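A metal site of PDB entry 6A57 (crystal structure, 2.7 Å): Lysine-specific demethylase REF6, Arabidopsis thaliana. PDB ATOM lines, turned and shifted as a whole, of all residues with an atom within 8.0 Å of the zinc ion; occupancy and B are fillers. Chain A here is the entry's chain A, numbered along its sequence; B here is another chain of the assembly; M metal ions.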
ATOM      1  N   LYS A  77      12.849 -14.439  22.119  1.00  0.00           N
ATOM      2  CA  LYS A  77      12.874 -13.371  23.126  1.00  0.00           C
ATOM      3  C   LYS A  77      12.626 -12.011  22.474  1.00  0.00           C
ATOM      4  O   LYS A  77      12.881 -11.842  21.278  1.00  0.00           O
ATOM      5  CB  LYS A  77      14.251 -13.320  23.799  1.00  0.00           C
ATOM      6  CG  LYS A  77      14.745 -14.630  24.401  1.00  0.00           C
ATOM      7  CD  LYS A  77      14.352 -14.791  25.861  1.00  0.00           C
ATOM      8  CE  LYS A  77      14.795 -16.131  26.420  1.00  0.00           C
ATOM      9  NZ  LYS A  77      13.857 -17.246  26.094  1.00  0.00           N
ATOM     10  N   CYS A  78      12.145 -11.049  23.250  1.00  0.00           N
ATOM     11  CA  CYS A  78      12.076  -9.667  22.804  1.00  0.00           C
ATOM     12  C   CYS A  78      13.390  -9.001  23.179  1.00  0.00           C
ATOM     13  O   CYS A  78      13.800  -9.108  24.330  1.00  0.00           O
ATOM     14  CB  CYS A  78      10.926  -8.909  23.467  1.00  0.00           C
ATOM     15  SG  CYS A  78      10.789  -7.189  22.922  1.00  0.00           S
ATOM     16  N   PRO A  79      14.034  -8.314  22.224  1.00  0.00           N
ATOM     17  CA  PRO A  79      15.344  -7.697  22.479  1.00  0.00           C
ATOM     18  C   PRO A  79      15.324  -6.317  23.166  1.00  0.00           C
ATOM     19  O   PRO A  79      16.404  -5.776  23.421  1.00  0.00           O
ATOM     20  CB  PRO A  79      15.932  -7.569  21.076  1.00  0.00           C
ATOM     21  CG  PRO A  79      14.745  -7.329  20.232  1.00  0.00           C
ATOM     22  CD  PRO A  79      13.649  -8.174  20.810  1.00  0.00           C
ATOM     23  N   TRP A  80      14.159  -5.749  23.480  1.00  0.00           N
ATOM     24  CA  TRP A  80      14.125  -4.458  24.187  1.00  0.00           C
ATOM     25  C   TRP A  80      14.528  -4.640  25.665  1.00  0.00           C
ATOM     26  O   TRP A  80      14.223  -5.672  26.268  1.00  0.00           O
ATOM     27  CB  TRP A  80      12.766  -3.741  24.035  1.00  0.00           C
ATOM     28  CG  TRP A  80      12.827  -2.589  23.047  1.00  0.00           C
ATOM     29  CD1 TRP A  80      12.785  -1.253  23.345  1.00  0.00           C
ATOM     30  CD2 TRP A  80      12.991  -2.672  21.623  1.00  0.00           C
ATOM     31  NE1 TRP A  80      12.892  -0.502  22.198  1.00  0.00           N
ATOM     32  CE2 TRP A  80      13.019  -1.343  21.120  1.00  0.00           C
ATOM     33  CE3 TRP A  80      13.099  -3.732  20.718  1.00  0.00           C
ATOM     34  CZ2 TRP A  80      13.166  -1.054  19.763  1.00  0.00           C
ATOM     35  CZ3 TRP A  80      13.236  -3.454  19.359  1.00  0.00           C
ATOM     36  CH2 TRP A  80      13.272  -2.119  18.893  1.00  0.00           C
ATOM     37  N   LYS A  81      15.205  -3.628  26.207  1.00  0.00           N
ATOM     38  CA  LYS A  81      15.964  -3.733  27.486  1.00  0.00           C
ATOM     39  C   LYS A  81      15.187  -4.364  28.644  1.00  0.00           C
ATOM     40  O   LYS A  81      15.522  -5.464  29.080  1.00  0.00           O
ATOM     41  CB  LYS A  81      16.498  -2.360  27.924  1.00  0.00           C
ATOM     42  N   GLY A  82      14.158  -3.682  29.112  1.00  0.00           N
ATOM     43  CA  GLY A  82      13.398  -4.152  30.280  1.00  0.00           C
ATOM     44  C   GLY A  82      12.255  -5.098  29.966  1.00  0.00           C
ATOM     45  O   GLY A  82      11.485  -5.442  30.873  1.00  0.00           O
ATOM     46  N   CYS A  83      12.127  -5.532  28.709  1.00  0.00           N
ATOM     47  CA  CYS A  83      10.975  -6.312  28.264  1.00  0.00           C
ATOM     48  C   CYS A  83      11.227  -7.817  28.406  1.00  0.00           C
ATOM     49  O   CYS A  83      12.122  -8.370  27.759  1.00  0.00           O
ATOM     50  CB  CYS A  83      10.640  -5.973  26.816  1.00  0.00           C
ATOM     51  SG  CYS A  83       9.067  -6.634  26.242  1.00  0.00           S
ATOM     52  N   LYS A  84      10.426  -8.466  29.248  1.00  0.00           N
ATOM     53  CA  LYS A  84      10.567  -9.913  29.529  1.00  0.00           C
ATOM     54  C   LYS A  84       9.764 -10.828  28.598  1.00  0.00           C
ATOM     55  O   LYS A  84       9.882 -12.053  28.697  1.00  0.00           O
ATOM     56  CB  LYS A  84      10.218 -10.220  31.007  1.00  0.00           C
ATOM     57  CG  LYS A  84      11.408 -10.535  31.909  1.00  0.00           C
ATOM     58  CD  LYS A  84      12.448  -9.424  32.017  1.00  0.00           C
ATOM     59  CE  LYS A  84      11.895  -8.169  32.681  1.00  0.00           C
ATOM     60  NZ  LYS A  84      11.327  -8.395  34.034  1.00  0.00           N
ATOM     61  N   MET A  85       8.960 -10.248  27.688  1.00  0.00           N
ATOM     62  CA  MET A  85       8.115 -11.036  26.771  1.00  0.00           C
ATOM     63  C   MET A  85       8.901 -12.121  26.030  1.00  0.00           C
ATOM     64  O   MET A  85      10.060 -11.922  25.651  1.00  0.00           O
ATOM     65  CB  MET A  85       7.427 -10.141  25.727  1.00  0.00           C
ATOM     66  CG  MET A  85       6.023  -9.682  26.104  1.00  0.00           C
ATOM     67  SD  MET A  85       4.817 -11.015  26.150  1.00  0.00           S
ATOM     68  CE  MET A  85       4.821 -11.638  24.481  1.00  0.00           C
ATOM     69  N   THR A  86       8.252 -13.270  25.853  1.00  0.00           N
ATOM     70  CA  THR A  86       8.831 -14.394  25.113  1.00  0.00           C
ATOM     71  C   THR A  86       7.768 -15.003  24.214  1.00  0.00           C
ATOM     72  O   THR A  86       6.587 -14.797  24.431  1.00  0.00           O
ATOM     73  CB  THR A  86       9.325 -15.488  26.055  1.00  0.00           C
ATOM     74  OG1 THR A  86       8.239 -15.936  26.883  1.00  0.00           O
ATOM     75  CG2 THR A  86      10.453 -14.969  26.942  1.00  0.00           C
ATOM     76  N   PHE A  87       8.222 -15.760  23.219  1.00  0.00           N
ATOM     77  CA  PHE A  87       7.349 -16.284  22.180  1.00  0.00           C
ATOM     78  C   PHE A  87       7.763 -17.679  21.768  1.00  0.00           C
ATOM     79  O   PHE A  87       8.905 -18.089  21.983  1.00  0.00           O
ATOM     80  CB  PHE A  87       7.391 -15.389  20.937  1.00  0.00           C
ATOM     81  CG  PHE A  87       7.328 -13.929  21.261  1.00  0.00           C
ATOM     82  CD1 PHE A  87       6.106 -13.273  21.334  1.00  0.00           C
ATOM     83  CD2 PHE A  87       8.495 -13.214  21.525  1.00  0.00           C
ATOM     84  CE1 PHE A  87       6.056 -11.941  21.637  1.00  0.00           C
ATOM     85  CE2 PHE A  87       8.440 -11.871  21.847  1.00  0.00           C
ATOM     86  CZ  PHE A  87       7.214 -11.229  21.906  1.00  0.00           C
ATOM     87  N   ARG A  93       6.590 -12.340  17.681  1.00  0.00           N
ATOM     88  CA  ARG A  93       7.756 -11.510  18.018  1.00  0.00           C
ATOM     89  C   ARG A  93       7.881 -10.269  17.112  1.00  0.00           C
ATOM     90  O   ARG A  93       8.094  -9.163  17.601  1.00  0.00           O
ATOM     91  CB  ARG A  93       9.043 -12.344  17.918  1.00  0.00           C
ATOM     92  CG  ARG A  93      10.309 -11.664  18.404  1.00  0.00           C
ATOM     93  CD  ARG A  93      11.488 -12.635  18.364  1.00  0.00           C
ATOM     94  NE  ARG A  93      12.744 -11.941  18.641  1.00  0.00           N
ATOM     95  CZ  ARG A  93      13.406 -11.178  17.763  1.00  0.00           C
ATOM     96  NH1 ARG A  93      12.963 -11.007  16.516  1.00  0.00           N
ATOM     97  NH2 ARG A  93      14.537 -10.574  18.143  1.00  0.00           N
ATOM     98  N   HIS A  96       5.085  -7.835  17.864  1.00  0.00           N
ATOM     99  CA  HIS A  96       5.292  -7.311  19.227  1.00  0.00           C
ATOM    100  C   HIS A  96       6.332  -6.202  19.294  1.00  0.00           C
ATOM    101  O   HIS A  96       6.175  -5.256  20.066  1.00  0.00           O
ATOM    102  CB  HIS A  96       5.664  -8.426  20.219  1.00  0.00           C
ATOM    103  CG  HIS A  96       6.264  -7.907  21.496  1.00  0.00           C
ATOM    104  ND1 HIS A  96       5.507  -7.639  22.612  1.00  0.00           N
ATOM    105  CD2 HIS A  96       7.540  -7.602  21.820  1.00  0.00           C
ATOM    106  CE1 HIS A  96       6.294  -7.196  23.580  1.00  0.00           C
ATOM    107  NE2 HIS A  96       7.536  -7.169  23.123  1.00  0.00           N
ATOM    108  N   ILE A  97       7.400  -6.326  18.517  1.00  0.00           N
ATOM    109  CA  ILE A  97       8.470  -5.330  18.560  1.00  0.00           C
ATOM    110  C   ILE A  97       7.928  -3.943  18.191  1.00  0.00           C
ATOM    111  O   ILE A  97       8.380  -2.931  18.729  1.00  0.00           O
ATOM    112  CB  ILE A  97       9.689  -5.731  17.691  1.00  0.00           C
ATOM    113  CG1 ILE A  97      10.412  -6.907  18.350  1.00  0.00           C
ATOM    114  CG2 ILE A  97      10.663  -4.570  17.540  1.00  0.00           C
ATOM    115  CD1 ILE A  97      11.340  -7.685  17.433  1.00  0.00           C
ATOM    116  N   ARG A  98       6.939  -3.906  17.299  1.00  0.00           N
ATOM    117  CA  ARG A  98       6.307  -2.646  16.905  1.00  0.00           C
ATOM    118  C   ARG A  98       5.748  -1.844  18.079  1.00  0.00           C
ATOM    119  O   ARG A  98       5.768  -0.617  18.045  1.00  0.00           O
ATOM    120  CB  ARG A  98       5.199  -2.885  15.885  1.00  0.00           C
ATOM    121  CG  ARG A  98       5.688  -3.362  14.540  1.00  0.00           C
ATOM    122  CD  ARG A  98       4.528  -3.773  13.670  1.00  0.00           C
ATOM    123  NE  ARG A  98       4.962  -4.669  12.615  1.00  0.00           N
ATOM    124  CZ  ARG A  98       4.216  -5.607  12.046  1.00  0.00           C
ATOM    125  NH1 ARG A  98       2.948  -5.830  12.416  1.00  0.00           N
ATOM    126  NH2 ARG A  98       4.740  -6.370  11.083  1.00  0.00           N
ATOM    127  N   VAL A  99       5.277  -2.536  19.112  1.00  0.00           N
ATOM    128  CA  VAL A  99       4.835  -1.872  20.350  1.00  0.00           C
ATOM    129  C   VAL A  99       5.928  -0.946  20.893  1.00  0.00           C
ATOM    130  O   VAL A  99       5.613   0.146  21.377  1.00  0.00           O
ATOM    131  CB  VAL A  99       4.428  -2.890  21.443  1.00  0.00           C
ATOM    132  CG1 VAL A  99       4.258  -2.218  22.808  1.00  0.00           C
ATOM    133  CG2 VAL A  99       3.148  -3.597  21.057  1.00  0.00           C
ATOM    134  N   HIS A 100       7.184  -1.375  20.818  1.00  0.00           N
ATOM    135  CA  HIS A 100       8.328  -0.572  21.284  1.00  0.00           C
ATOM    136  C   HIS A 100       8.702   0.526  20.290  1.00  0.00           C
ATOM    137  O   HIS A 100       8.897   1.676  20.697  1.00  0.00           O
ATOM    138  CB  HIS A 100       9.546  -1.468  21.556  1.00  0.00           C
ATOM    139  CG  HIS A 100       9.310  -2.504  22.614  1.00  0.00           C
ATOM    140  ND1 HIS A 100       9.118  -2.183  23.942  1.00  0.00           N
ATOM    141  CD2 HIS A 100       9.223  -3.853  22.542  1.00  0.00           C
ATOM    142  CE1 HIS A 100       8.924  -3.293  24.637  1.00  0.00           C
ATOM    143  NE2 HIS A 100       8.981  -4.320  23.812  1.00  0.00           N
ATOM    144  P    DT B   6       1.914  -8.197  21.745  1.00  0.00           P
ATOM    145  OP1  DT B   6       3.011  -8.179  22.727  1.00  0.00           O
ATOM    146  OP2  DT B   6       2.182  -7.834  20.330  1.00  0.00           O
ATOM    147  O5'  DT B   6       1.222  -9.634  21.716  1.00  0.00           O
ATOM    148  C5'  DT B   6       0.870 -10.282  22.933  1.00  0.00           C
ATOM    149  C4'  DT B   6       0.210 -11.601  22.627  1.00  0.00           C
ATOM    150  O4'  DT B   6      -0.909 -11.379  21.742  1.00  0.00           O
ATOM    151  C3'  DT B   6       1.111 -12.629  21.931  1.00  0.00           C
ATOM    152  O3'  DT B   6       0.958 -13.900  22.589  1.00  0.00           O
ATOM    153  C2'  DT B   6       0.624 -12.606  20.498  1.00  0.00           C
ATOM    154  C1'  DT B   6      -0.862 -12.306  20.681  1.00  0.00           C
ATOM    155  N1   DT B   6      -1.561 -11.724  19.519  1.00  0.00           N
ATOM    156  C2   DT B   6      -2.701 -12.338  19.038  1.00  0.00           C
ATOM    157  O2   DT B   6      -3.155 -13.359  19.525  1.00  0.00           O
ATOM    158  N3   DT B   6      -3.275 -11.717  17.966  1.00  0.00           N
ATOM    159  C4   DT B   6      -2.859 -10.560  17.342  1.00  0.00           C
ATOM    160  O4   DT B   6      -3.487 -10.123  16.388  1.00  0.00           O
ATOM    161  C5   DT B   6      -1.666  -9.964  17.898  1.00  0.00           C
ATOM    162  C7   DT B   6      -1.138  -8.707  17.279  1.00  0.00           C
ATOM    163  C6   DT B   6      -1.093 -10.558  18.946  1.00  0.00           C
HETATM  164 ZN    ZN M   1       9.100  -6.358  24.062  1.00  0.00          ZN
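ND1 of His 96 is in hydrogen-bond range of OP1 of DT 6 of chain B (2.6 Å). O of Met 85 is in hydrogen-bond range of N of Cys 78 (3.3 Å). SG of Cys 78 sits close to N of Trp 80.
Of the 18 residues printed, 4 come within 4 Å of the zinc ion. Along chain A the residues within 4 Å of the zinc ion span positions 78 to 100. The nearest printed residue that does not touch the zinc ion is Met 85 (4.5 Å).
The zinc ion is bound by NE2 of His 96, 2.0 Å away. NE2 of His 100 is bound to the zinc ion, 2.1 Å away. The side-chain sulfur (SG) of Cys 83 binds the zinc ion, at 2.2 Å. The zinc ion is bound by SG of Cys 78, 2.2 Å away.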
